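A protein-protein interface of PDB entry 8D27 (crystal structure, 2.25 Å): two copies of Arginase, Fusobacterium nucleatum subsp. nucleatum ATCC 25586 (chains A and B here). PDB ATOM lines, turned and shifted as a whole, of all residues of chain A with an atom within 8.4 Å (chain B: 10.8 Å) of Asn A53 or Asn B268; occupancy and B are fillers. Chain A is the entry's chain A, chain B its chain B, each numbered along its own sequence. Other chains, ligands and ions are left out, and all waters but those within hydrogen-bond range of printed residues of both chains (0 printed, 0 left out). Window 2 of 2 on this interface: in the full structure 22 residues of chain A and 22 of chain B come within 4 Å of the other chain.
Hydrophobic or aromatic side chains of chain B that line the printed part of chain A: Leu B264. Among the printed residues, 8 pairs touch across the chains. Among the printed residues, no Asp or Glu carboxylate lies within 4 Å of a Lys or Arg side-chain nitrogen of the other chain.
The backbone NH (N) of Asn B268 sits close to the side-chain amide nitrogen (ND2) of Asn A53, at 3.4 Å. The side-chain amino group (NZ) of Lys A55 lies within hydrogen-bond range of the backbone carbonyl oxygen (O) of Leu B264 (2.9 Å). The backbone carbonyl oxygen (O) of Asp B266 is in hydrogen-bond range of the side-chain amino group (NZ) of Lys A55, at 3.2 Å.
Among the printed residues, merely in contact across the chains: Phe A52 with Asp B28 (3.6 Å), Phe A52 with Pro B263 (3.6 Å), Phe A52 with Leu B264 (3.7 Å), Lys A55 with Asn B265 (3.7 Å) and Lys A58 with Leu B264 (3.98 Å).
The side-chain carboxylate (OD1) of Asp A51 lies close to the backbone NH (N) of Asn A53. The side-chain amide oxygen (OD1) of Asn B262 lies close to the backbone NH (N) of Leu B264. OD1 of Asn B262 sits close to OD1 of Asn B265, 3.4 Å away. The side-chain carboxylate (OD1) of Asp B266 is in hydrogen-bond range of the side-chain hydroxyl (OG1) of Thr B271. The backbone NH (N) of Ala B272 is in hydrogen-bond range of the side-chain carboxylate (OD2) of Asp B266 (3.2 Å).
Asn A53 touches just one residue of chain B: Asn B268. Of chain A, only Asn A53 (3.4 Å) comes within 4 Å of Asn B268. Of chain B, only Leu B264, Asn B265 and Asp B266 come within 4 Å of Lys A55. No residue of chain A comes within 4 Å of Gly B269. Of the printed residues of chain A, Asp B28 touches Phe A52 (3.6 Å). Printed residues of chain B within 4 Å of Phe A52: Asp B28 (3.6 Å), Pro B263 (3.6 Å) and Leu B264 (3.7 Å). Of the printed residues of chain B, Lys A58 touches Leu B264. Ala B272 touches none of the printed residues of chain A.
No position is printed for both chains.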
ATOM      1  N   LYS A  49     -23.761  -7.414  22.064  1.00  0.00           N
ATOM      2  CA  LYS A  49     -22.505  -7.942  21.545  1.00  0.00           C
ATOM      3  C   LYS A  49     -22.731  -9.337  20.980  1.00  0.00           C
ATOM      4  O   LYS A  49     -23.354 -10.187  21.622  1.00  0.00           O
ATOM      5  CB  LYS A  49     -21.456  -7.959  22.661  1.00  0.00           C
ATOM      6  CG  LYS A  49     -20.423  -9.073  22.581  1.00  0.00           C
ATOM      7  CD  LYS A  49     -19.439  -8.854  21.448  1.00  0.00           C
ATOM      8  CE  LYS A  49     -18.499 -10.037  21.310  1.00  0.00           C
ATOM      9  NZ  LYS A  49     -17.797 -10.039  20.000  1.00  0.00           N
ATOM     10  N   GLU A  50     -22.214  -9.573  19.778  1.00  0.00           N
ATOM     11  CA  GLU A  50     -22.424 -10.819  19.058  1.00  0.00           C
ATOM     12  C   GLU A  50     -21.089 -11.489  18.755  1.00  0.00           C
ATOM     13  O   GLU A  50     -20.015 -10.910  18.937  1.00  0.00           O
ATOM     14  CB  GLU A  50     -23.180 -10.579  17.744  1.00  0.00           C
ATOM     15  CG  GLU A  50     -24.610 -10.085  17.894  1.00  0.00           C
ATOM     16  CD  GLU A  50     -25.411 -10.883  18.898  1.00  0.00           C
ATOM     17  OE1 GLU A  50     -25.270 -12.121  18.928  1.00  0.00           O
ATOM     18  OE2 GLU A  50     -26.196 -10.269  19.648  1.00  0.00           O
ATOM     19  N   ASP A  51     -21.177 -12.731  18.287  1.00  0.00           N
ATOM     20  CA  ASP A  51     -20.046 -13.460  17.723  1.00  0.00           C
ATOM     21  C   ASP A  51     -20.332 -13.609  16.231  1.00  0.00           C
ATOM     22  O   ASP A  51     -20.845 -14.632  15.771  1.00  0.00           O
ATOM     23  CB  ASP A  51     -19.849 -14.815  18.388  1.00  0.00           C
ATOM     24  CG  ASP A  51     -18.779 -15.647  17.705  1.00  0.00           C
ATOM     25  OD1 ASP A  51     -18.000 -15.078  16.910  1.00  0.00           O
ATOM     26  OD2 ASP A  51     -18.717 -16.868  17.957  1.00  0.00           O
ATOM     27  N   PHE A  52     -20.004 -12.566  15.469  1.00  0.00           N
ATOM     28  CA  PHE A  52     -20.262 -12.567  14.036  1.00  0.00           C
ATOM     29  C   PHE A  52     -19.423 -13.589  13.288  1.00  0.00           C
ATOM     30  O   PHE A  52     -19.569 -13.709  12.066  1.00  0.00           O
ATOM     31  CB  PHE A  52     -20.022 -11.172  13.469  1.00  0.00           C
ATOM     32  CG  PHE A  52     -21.107 -10.194  13.809  1.00  0.00           C
ATOM     33  CD1 PHE A  52     -22.341 -10.265  13.186  1.00  0.00           C
ATOM     34  CD2 PHE A  52     -20.896  -9.208  14.755  1.00  0.00           C
ATOM     35  CE1 PHE A  52     -23.342  -9.365  13.497  1.00  0.00           C
ATOM     36  CE2 PHE A  52     -21.894  -8.307  15.070  1.00  0.00           C
ATOM     37  CZ  PHE A  52     -23.118  -8.385  14.441  1.00  0.00           C
ATOM     38  N   ASN A  53     -18.553 -14.317  13.980  1.00  0.00           N
ATOM     39  CA  ASN A  53     -17.891 -15.474  13.402  1.00  0.00           C
ATOM     40  C   ASN A  53     -18.728 -16.736  13.520  1.00  0.00           C
ATOM     41  O   ASN A  53     -18.485 -17.701  12.787  1.00  0.00           O
ATOM     42  CB  ASN A  53     -16.539 -15.695  14.078  1.00  0.00           C
ATOM     43  CG  ASN A  53     -15.466 -14.805  13.511  1.00  0.00           C
ATOM     44  OD1 ASN A  53     -15.060 -13.827  14.138  1.00  0.00           O
ATOM     45  ND2 ASN A  53     -15.003 -15.130  12.308  1.00  0.00           N
ATOM     46  N   ASP A  54     -19.701 -16.751  14.427  1.00  0.00           N
ATOM     47  CA  ASP A  54     -20.676 -17.835  14.511  1.00  0.00           C
ATOM     48  C   ASP A  54     -21.801 -17.509  13.539  1.00  0.00           C
ATOM     49  O   ASP A  54     -22.775 -16.838  13.881  1.00  0.00           O
ATOM     50  CB  ASP A  54     -21.188 -17.992  15.934  1.00  0.00           C
ATOM     51  CG  ASP A  54     -22.012 -19.246  16.114  1.00  0.00           C
ATOM     52  OD1 ASP A  54     -22.235 -19.960  15.112  1.00  0.00           O
ATOM     53  OD2 ASP A  54     -22.436 -19.517  17.255  1.00  0.00           O
ATOM     54  N   LYS A  55     -21.663 -17.985  12.305  1.00  0.00           N
ATOM     55  CA  LYS A  55     -22.612 -17.676  11.244  1.00  0.00           C
ATOM     56  C   LYS A  55     -23.707 -18.723  11.109  1.00  0.00           C
ATOM     57  O   LYS A  55     -24.499 -18.654  10.164  1.00  0.00           O
ATOM     58  CB  LYS A  55     -21.872 -17.517   9.916  1.00  0.00           C
ATOM     59  CG  LYS A  55     -20.807 -16.433   9.953  1.00  0.00           C
ATOM     60  CD  LYS A  55     -20.000 -16.384   8.671  1.00  0.00           C
ATOM     61  CE  LYS A  55     -19.258 -15.062   8.550  1.00  0.00           C
ATOM     62  NZ  LYS A  55     -20.063 -14.033   7.830  1.00  0.00           N
ATOM     63  N   LYS A  56     -23.765 -19.690  12.019  1.00  0.00           N
ATOM     64  CA  LYS A  56     -24.874 -20.628  12.093  1.00  0.00           C
ATOM     65  C   LYS A  56     -25.871 -20.257  13.181  1.00  0.00           C
ATOM     66  O   LYS A  56     -26.883 -20.943  13.338  1.00  0.00           O
ATOM     67  CB  LYS A  56     -24.346 -22.045  12.331  1.00  0.00           C
ATOM     68  CG  LYS A  56     -23.908 -22.752  11.055  1.00  0.00           C
ATOM     69  CD  LYS A  56     -22.809 -23.765  11.323  1.00  0.00           C
ATOM     70  CE  LYS A  56     -22.505 -24.588  10.080  1.00  0.00           C
ATOM     71  NZ  LYS A  56     -21.303 -25.451  10.252  1.00  0.00           N
ATOM     72  N   LEU A  57     -25.614 -19.179  13.924  1.00  0.00           N
ATOM     73  CA  LEU A  57     -26.451 -18.731  15.031  1.00  0.00           C
ATOM     74  C   LEU A  57     -26.366 -17.202  15.062  1.00  0.00           C
ATOM     75  O   LEU A  57     -25.838 -16.585  15.986  1.00  0.00           O
ATOM     76  CB  LEU A  57     -26.002 -19.354  16.352  1.00  0.00           C
ATOM     77  CG  LEU A  57     -27.027 -19.419  17.482  1.00  0.00           C
ATOM     78  CD1 LEU A  57     -28.184 -20.323  17.111  1.00  0.00           C
ATOM     79  CD2 LEU A  57     -26.356 -19.904  18.753  1.00  0.00           C
ATOM     80  N   LYS A  58     -26.913 -16.576  14.022  1.00  0.00           N
ATOM     81  CA  LYS A  58     -26.694 -15.156  13.778  1.00  0.00           C
ATOM     82  C   LYS A  58     -27.532 -14.297  14.715  1.00  0.00           C
ATOM     83  O   LYS A  58     -28.739 -14.510  14.861  1.00  0.00           O
ATOM     84  CB  LYS A  58     -27.019 -14.826  12.322  1.00  0.00           C
ATOM     85  CG  LYS A  58     -26.084 -15.500  11.331  1.00  0.00           C
ATOM     86  CD  LYS A  58     -26.671 -15.530   9.933  1.00  0.00           C
ATOM     87  CE  LYS A  58     -25.576 -15.672   8.892  1.00  0.00           C
ATOM     88  NZ  LYS A  58     -26.085 -16.245   7.618  1.00  0.00           N
ATOM     89  N   LYS A  60     -27.263 -14.126  18.037  1.00  0.00           N
ATOM     90  CA  LYS A  60     -27.700 -14.966  19.145  1.00  0.00           C
ATOM     91  C   LYS A  60     -28.133 -14.115  20.332  1.00  0.00           C
ATOM     92  O   LYS A  60     -29.279 -14.184  20.781  1.00  0.00           O
ATOM     93  CB  LYS A  60     -26.582 -15.925  19.561  1.00  0.00           C
ATOM     94  CG  LYS A  60     -26.713 -16.425  21.003  1.00  0.00           C
ATOM     95  CD  LYS A  60     -25.697 -17.508  21.341  1.00  0.00           C
ATOM     96  CE  LYS A  60     -24.271 -16.992  21.233  1.00  0.00           C
ATOM     97  NZ  LYS A  60     -23.624 -17.411  19.957  1.00  0.00           N
ATOM     98  N   ASP B  28     -20.849  -2.603  16.823  1.00  0.00           N
ATOM     99  CA  ASP B  28     -19.846  -3.666  16.670  1.00  0.00           C
ATOM    100  C   ASP B  28     -18.479  -3.070  16.936  1.00  0.00           C
ATOM    101  O   ASP B  28     -17.773  -3.733  17.600  1.00  0.00           O
ATOM    102  CB  ASP B  28     -19.825  -4.332  15.293  1.00  0.00           C
ATOM    103  CG  ASP B  28     -18.719  -5.357  15.139  1.00  0.00           C
ATOM    104  OD1 ASP B  28     -18.842  -6.423  15.745  1.00  0.00           O
ATOM    105  OD2 ASP B  28     -17.738  -5.063  14.440  1.00  0.00           O
ATOM    106  N   LEU B  29     -18.158  -1.895  16.371  1.00  0.00           N
ATOM    107  CA  LEU B  29     -16.834  -1.297  16.494  1.00  0.00           C
ATOM    108  C   LEU B  29     -16.572  -0.832  17.921  1.00  0.00           C
ATOM    109  O   LEU B  29     -15.476  -1.043  18.457  1.00  0.00           O
ATOM    110  CB  LEU B  29     -16.691  -0.150  15.498  1.00  0.00           C
ATOM    111  CG  LEU B  29     -16.685  -0.652  14.049  1.00  0.00           C
ATOM    112  CD1 LEU B  29     -17.138   0.425  13.076  1.00  0.00           C
ATOM    113  CD2 LEU B  29     -15.307  -1.185  13.667  1.00  0.00           C
ATOM    114  N   ALA B  32     -15.390  -3.867  19.306  1.00  0.00           N
ATOM    115  CA  ALA B  32     -14.235  -4.516  18.701  1.00  0.00           C
ATOM    116  C   ALA B  32     -12.954  -3.745  18.989  1.00  0.00           C
ATOM    117  O   ALA B  32     -11.901  -4.349  19.217  1.00  0.00           O
ATOM    118  CB  ALA B  32     -14.445  -4.667  17.193  1.00  0.00           C
ATOM    119  N   TYR B  33     -13.026  -2.415  18.994  1.00  0.00           N
ATOM    120  CA  TYR B  33     -11.863  -1.556  19.224  1.00  0.00           C
ATOM    121  C   TYR B  33     -12.279  -0.411  20.135  1.00  0.00           C
ATOM    122  O   TYR B  33     -12.362   0.748  19.712  1.00  0.00           O
ATOM    123  CB  TYR B  33     -11.302  -1.036  17.899  1.00  0.00           C
ATOM    124  CG  TYR B  33     -11.246  -2.077  16.802  1.00  0.00           C
ATOM    125  CD1 TYR B  33     -10.209  -2.997  16.744  1.00  0.00           C
ATOM    126  CD2 TYR B  33     -12.227  -2.134  15.822  1.00  0.00           C
ATOM    127  CE1 TYR B  33     -10.153  -3.946  15.742  1.00  0.00           C
ATOM    128  CE2 TYR B  33     -12.180  -3.079  14.818  1.00  0.00           C
ATOM    129  CZ  TYR B  33     -11.141  -3.981  14.782  1.00  0.00           C
ATOM    130  OH  TYR B  33     -11.091  -4.922  13.784  1.00  0.00           O
ATOM    131  N   PRO B 221     -13.497  -7.352  -2.638  1.00  0.00           N
ATOM    132  CA  PRO B 221     -14.267  -8.142  -1.665  1.00  0.00           C
ATOM    133  C   PRO B 221     -13.455  -9.199  -0.940  1.00  0.00           C
ATOM    134  O   PRO B 221     -13.903  -9.686   0.105  1.00  0.00           O
ATOM    135  CB  PRO B 221     -15.371  -8.774  -2.525  1.00  0.00           C
ATOM    136  CG  PRO B 221     -15.548  -7.820  -3.648  1.00  0.00           C
ATOM    137  CD  PRO B 221     -14.155  -7.328  -3.958  1.00  0.00           C
ATOM    138  N   GLU B 222     -12.283  -9.582  -1.451  1.00  0.00           N
ATOM    139  CA  GLU B 222     -11.446 -10.521  -0.716  1.00  0.00           C
ATOM    140  C   GLU B 222     -10.823  -9.879   0.516  1.00  0.00           C
ATOM    141  O   GLU B 222     -10.478 -10.589   1.465  1.00  0.00           O
ATOM    142  CB  GLU B 222     -10.347 -11.085  -1.621  1.00  0.00           C
ATOM    143  CG  GLU B 222      -9.634 -10.054  -2.475  1.00  0.00           C
ATOM    144  CD  GLU B 222     -10.104 -10.074  -3.914  1.00  0.00           C
ATOM    145  OE1 GLU B 222     -11.287  -9.753  -4.155  1.00  0.00           O
ATOM    146  OE2 GLU B 222      -9.293 -10.407  -4.805  1.00  0.00           O
ATOM    147  N   ILE B 223     -10.681  -8.557   0.521  1.00  0.00           N
ATOM    148  CA  ILE B 223     -10.136  -7.832   1.656  1.00  0.00           C
ATOM    149  C   ILE B 223     -11.239  -7.287   2.552  1.00  0.00           C
ATOM    150  O   ILE B 223     -11.095  -7.265   3.774  1.00  0.00           O
ATOM    151  CB  ILE B 223      -9.213  -6.694   1.164  1.00  0.00           C
ATOM    152  CG1 ILE B 223      -8.314  -7.179   0.025  1.00  0.00           C
ATOM    153  CG2 ILE B 223      -8.365  -6.156   2.309  1.00  0.00           C
ATOM    154  CD1 ILE B 223      -7.569  -8.467   0.326  1.00  0.00           C
ATOM    155  N   ALA B 224     -12.347  -6.837   1.956  1.00  0.00           N
ATOM    156  CA  ALA B 224     -13.484  -6.278   2.684  1.00  0.00           C
ATOM    157  C   ALA B 224     -14.713  -7.111   2.350  1.00  0.00           C
ATOM    158  O   ALA B 224     -15.578  -6.683   1.566  1.00  0.00           O
ATOM    159  CB  ALA B 224     -13.702  -4.806   2.337  1.00  0.00           C
ATOM    160  N   PRO B 225     -14.825  -8.316   2.917  1.00  0.00           N
ATOM    161  CA  PRO B 225     -16.022  -9.130   2.653  1.00  0.00           C
ATOM    162  C   PRO B 225     -17.279  -8.571   3.288  1.00  0.00           C
ATOM    163  O   PRO B 225     -18.363  -8.683   2.704  1.00  0.00           O
ATOM    164  CB  PRO B 225     -15.647 -10.498   3.239  1.00  0.00           C
ATOM    165  CG  PRO B 225     -14.645 -10.177   4.308  1.00  0.00           C
ATOM    166  CD  PRO B 225     -13.852  -9.016   3.776  1.00  0.00           C
ATOM    167  N   GLY B 226     -17.166  -7.967   4.470  1.00  0.00           N
ATOM    168  CA  GLY B 226     -18.325  -7.485   5.196  1.00  0.00           C
ATOM    169  C   GLY B 226     -18.972  -6.230   4.642  1.00  0.00           C
ATOM    170  O   GLY B 226     -18.907  -5.167   5.266  1.00  0.00           O
ATOM    171  N   PHE B 261     -20.323  -0.638   6.436  1.00  0.00           N
ATOM    172  CA  PHE B 261     -19.635  -1.735   7.102  1.00  0.00           C
ATOM    173  C   PHE B 261     -20.689  -2.706   7.616  1.00  0.00           C
ATOM    174  O   PHE B 261     -21.413  -2.402   8.571  1.00  0.00           O
ATOM    175  CB  PHE B 261     -18.758  -1.225   8.237  1.00  0.00           C
ATOM    176  CG  PHE B 261     -18.329  -2.300   9.192  1.00  0.00           C
ATOM    177  CD1 PHE B 261     -17.715  -3.455   8.733  1.00  0.00           C
ATOM    178  CD2 PHE B 261     -18.544  -2.156  10.551  1.00  0.00           C
ATOM    179  CE1 PHE B 261     -17.324  -4.441   9.613  1.00  0.00           C
ATOM    180  CE2 PHE B 261     -18.154  -3.135  11.435  1.00  0.00           C
ATOM    181  CZ  PHE B 261     -17.543  -4.281  10.967  1.00  0.00           C
ATOM    182  N   ASN B 262     -20.784  -3.868   6.972  1.00  0.00           N
ATOM    183  CA  ASN B 262     -21.742  -4.894   7.350  1.00  0.00           C
ATOM    184  C   ASN B 262     -21.025  -5.948   8.178  1.00  0.00           C
ATOM    185  O   ASN B 262     -20.349  -6.820   7.612  1.00  0.00           O
ATOM    186  CB  ASN B 262     -22.374  -5.522   6.108  1.00  0.00           C
ATOM    187  CG  ASN B 262     -23.684  -6.206   6.411  1.00  0.00           C
ATOM    188  OD1 ASN B 262     -23.727  -7.178   7.164  1.00  0.00           O
ATOM    189  ND2 ASN B 262     -24.765  -5.697   5.835  1.00  0.00           N
ATOM    190  N   PRO B 263     -21.115  -5.908   9.511  1.00  0.00           N
ATOM    191  CA  PRO B 263     -20.406  -6.915  10.319  1.00  0.00           C
ATOM    192  C   PRO B 263     -20.931  -8.334  10.146  1.00  0.00           C
ATOM    193  O   PRO B 263     -20.191  -9.285  10.426  1.00  0.00           O
ATOM    194  CB  PRO B 263     -20.608  -6.419  11.761  1.00  0.00           C
ATOM    195  CG  PRO B 263     -21.783  -5.483  11.694  1.00  0.00           C
ATOM    196  CD  PRO B 263     -21.720  -4.851  10.341  1.00  0.00           C
ATOM    197  N   LEU B 264     -22.173  -8.509   9.689  1.00  0.00           N
ATOM    198  CA  LEU B 264     -22.732  -9.852   9.574  1.00  0.00           C
ATOM    199  C   LEU B 264     -22.004 -10.667   8.514  1.00  0.00           C
ATOM    200  O   LEU B 264     -21.779 -11.870   8.695  1.00  0.00           O
ATOM    201  CB  LEU B 264     -24.223  -9.769   9.252  1.00  0.00           C
ATOM    202  CG  LEU B 264     -24.996 -11.088   9.226  1.00  0.00           C
ATOM    203  CD1 LEU B 264     -25.012 -11.739  10.597  1.00  0.00           C
ATOM    204  CD2 LEU B 264     -26.415 -10.863   8.728  1.00  0.00           C
ATOM    205  N   ASN B 265     -21.638 -10.037   7.402  1.00  0.00           N
ATOM    206  CA  ASN B 265     -20.933 -10.712   6.323  1.00  0.00           C
ATOM    207  C   ASN B 265     -19.419 -10.641   6.473  1.00  0.00           C
ATOM    208  O   ASN B 265     -18.699 -11.090   5.575  1.00  0.00           O
ATOM    209  CB  ASN B 265     -21.339 -10.116   4.972  1.00  0.00           C
ATOM    210  CG  ASN B 265     -22.830 -10.210   4.718  1.00  0.00           C
ATOM    211  OD1 ASN B 265     -23.634 -10.187   5.648  1.00  0.00           O
ATOM    212  ND2 ASN B 265     -23.207 -10.319   3.449  1.00  0.00           N
ATOM    213  N   ASP B 266     -18.921 -10.089   7.576  1.00  0.00           N
ATOM    214  CA  ASP B 266     -17.486  -9.956   7.766  1.00  0.00           C
ATOM    215  C   ASP B 266     -16.880 -11.297   8.162  1.00  0.00           C
ATOM    216  O   ASP B 266     -17.560 -12.194   8.664  1.00  0.00           O
ATOM    217  CB  ASP B 266     -17.175  -8.899   8.829  1.00  0.00           C
ATOM    218  CG  ASP B 266     -15.737  -8.395   8.757  1.00  0.00           C
ATOM    219  OD1 ASP B 266     -15.022  -8.725   7.786  1.00  0.00           O
ATOM    220  OD2 ASP B 266     -15.321  -7.666   9.682  1.00  0.00           O
ATOM    221  N   ILE B 267     -15.581 -11.421   7.930  1.00  0.00           N
ATOM    222  CA  ILE B 267     -14.856 -12.669   8.151  1.00  0.00           C
ATOM    223  C   ILE B 267     -13.705 -12.354   9.099  1.00  0.00           C
ATOM    224  O   ILE B 267     -12.596 -12.018   8.676  1.00  0.00           O
ATOM    225  CB  ILE B 267     -14.359 -13.291   6.842  1.00  0.00           C
ATOM    226  CG1 ILE B 267     -15.550 -13.735   5.985  1.00  0.00           C
ATOM    227  CG2 ILE B 267     -13.444 -14.473   7.122  1.00  0.00           C
ATOM    228  CD1 ILE B 267     -15.221 -13.919   4.518  1.00  0.00           C
ATOM    229  N   ASN B 268     -13.972 -12.458  10.404  1.00  0.00           N
ATOM    230  CA  ASN B 268     -12.940 -12.367  11.437  1.00  0.00           C
ATOM    231  C   ASN B 268     -12.451 -10.934  11.623  1.00  0.00           C
ATOM    232  O   ASN B 268     -11.276 -10.695  11.901  1.00  0.00           O
ATOM    233  CB  ASN B 268     -11.767 -13.302  11.122  1.00  0.00           C
ATOM    234  CG  ASN B 268     -11.079 -13.828  12.373  1.00  0.00           C
ATOM    235  OD1 ASN B 268     -11.625 -13.770  13.474  1.00  0.00           O
ATOM    236  ND2 ASN B 268      -9.871 -14.348  12.202  1.00  0.00           N
ATOM    237  N   GLY B 269     -13.357  -9.970  11.478  1.00  0.00           N
ATOM    238  CA  GLY B 269     -13.006  -8.578  11.673  1.00  0.00           C
ATOM    239  C   GLY B 269     -12.043  -7.995  10.666  1.00  0.00           C
ATOM    240  O   GLY B 269     -11.503  -6.912  10.910  1.00  0.00           O
ATOM    241  N   LYS B 270     -11.804  -8.677   9.545  1.00  0.00           N
ATOM    242  CA  LYS B 270     -10.930  -8.134   8.510  1.00  0.00           C
ATOM    243  C   LYS B 270     -11.422  -6.768   8.045  1.00  0.00           C
ATOM    244  O   LYS B 270     -10.666  -5.787   8.022  1.00  0.00           O
ATOM    245  CB  LYS B 270     -10.855  -9.119   7.338  1.00  0.00           C
ATOM    246  CG  LYS B 270     -10.040 -10.369   7.648  1.00  0.00           C
ATOM    247  CD  LYS B 270     -10.031 -11.418   6.525  1.00  0.00           C
ATOM    248  CE  LYS B 270     -11.203 -11.309   5.562  1.00  0.00           C
ATOM    249  NZ  LYS B 270     -11.245 -12.473   4.626  1.00  0.00           N
ATOM    250  N   THR B 271     -12.701  -6.690   7.675  1.00  0.00           N
ATOM    251  CA  THR B 271     -13.303  -5.413   7.312  1.00  0.00           C
ATOM    252  C   THR B 271     -13.340  -4.464   8.502  1.00  0.00           C
ATOM    253  O   THR B 271     -13.099  -3.258   8.359  1.00  0.00           O
ATOM    254  CB  THR B 271     -14.716  -5.649   6.777  1.00  0.00           C
ATOM    255  OG1 THR B 271     -14.688  -6.673   5.773  1.00  0.00           O
ATOM    256  CG2 THR B 271     -15.288  -4.376   6.183  1.00  0.00           C
ATOM    257  N   ALA B 272     -13.663  -4.986   9.686  1.00  0.00           N
ATOM    258  CA  ALA B 272     -13.671  -4.137  10.869  1.00  0.00           C
ATOM    259  C   ALA B 272     -12.286  -3.573  11.141  1.00  0.00           C
ATOM    260  O   ALA B 272     -12.162  -2.435  11.600  1.00  0.00           O
ATOM    261  CB  ALA B 272     -14.181  -4.917  12.080  1.00  0.00           C
ATOM    262  N   GLU B 273     -11.233  -4.339  10.845  1.00  0.00           N
ATOM    263  CA  GLU B 273      -9.884  -3.815  11.024  1.00  0.00           C
ATOM    264  C   GLU B 273      -9.554  -2.782   9.955  1.00  0.00           C
ATOM    265  O   GLU B 273      -8.847  -1.805  10.230  1.00  0.00           O
ATOM    266  CB  GLU B 273      -8.862  -4.946  10.998  1.00  0.00           C
ATOM    267  CG  GLU B 273      -7.550  -4.581  11.670  1.00  0.00           C
ATOM    268  CD  GLU B 273      -7.658  -4.574  13.183  1.00  0.00           C
ATOM    269  OE1 GLU B 273      -7.331  -3.536  13.799  1.00  0.00           O
ATOM    270  OE2 GLU B 273      -8.072  -5.607  13.754  1.00  0.00           O
ATOM    271  N   LEU B 274     -10.042  -2.984   8.729  1.00  0.00           N
ATOM    272  CA  LEU B 274      -9.921  -1.934   7.721  1.00  0.00           C
ATOM    273  C   LEU B 274     -10.501  -0.627   8.248  1.00  0.00           C
ATOM    274  O   LEU B 274      -9.882   0.438   8.141  1.00  0.00           O
ATOM    275  CB  LEU B 274     -10.633  -2.345   6.434  1.00  0.00           C
ATOM    276  CG  LEU B 274      -9.907  -3.309   5.498  1.00  0.00           C
ATOM    277  CD1 LEU B 274     -10.800  -3.673   4.318  1.00  0.00           C
ATOM    278  CD2 LEU B 274      -8.601  -2.713   5.014  1.00  0.00           C
ATOM    279  N   VAL B 275     -11.700  -0.697   8.827  1.00  0.00           N
ATOM    280  CA  VAL B 275     -12.356   0.515   9.310  1.00  0.00           C
ATOM    281  C   VAL B 275     -11.610   1.086  10.510  1.00  0.00           C
ATOM    282  O   VAL B 275     -11.470   2.308  10.652  1.00  0.00           O
ATOM    283  CB  VAL B 275     -13.830   0.231   9.641  1.00  0.00           C
ATOM    284  CG1 VAL B 275     -14.461   1.437  10.317  1.00  0.00           C
ATOM    285  CG2 VAL B 275     -14.587  -0.129   8.379  1.00  0.00           C
ATOM    286  N   ASN B 276     -11.124   0.215  11.395  1.00  0.00           N
ATOM    287  CA  ASN B 276     -10.317   0.669  12.521  1.00  0.00           C
ATOM    288  C   ASN B 276      -9.110   1.463  12.039  1.00  0.00           C
ATOM    289  O   ASN B 276      -8.823   2.549  12.550  1.00  0.00           O
ATOM    290  CB  ASN B 276      -9.874  -0.533  13.354  1.00  0.00           C
ATOM    291  CG  ASN B 276      -9.182  -0.128  14.637  1.00  0.00           C
ATOM    292  OD1 ASN B 276      -9.661   0.739  15.367  1.00  0.00           O
ATOM    293  ND2 ASN B 276      -8.047  -0.756  14.920  1.00  0.00           N
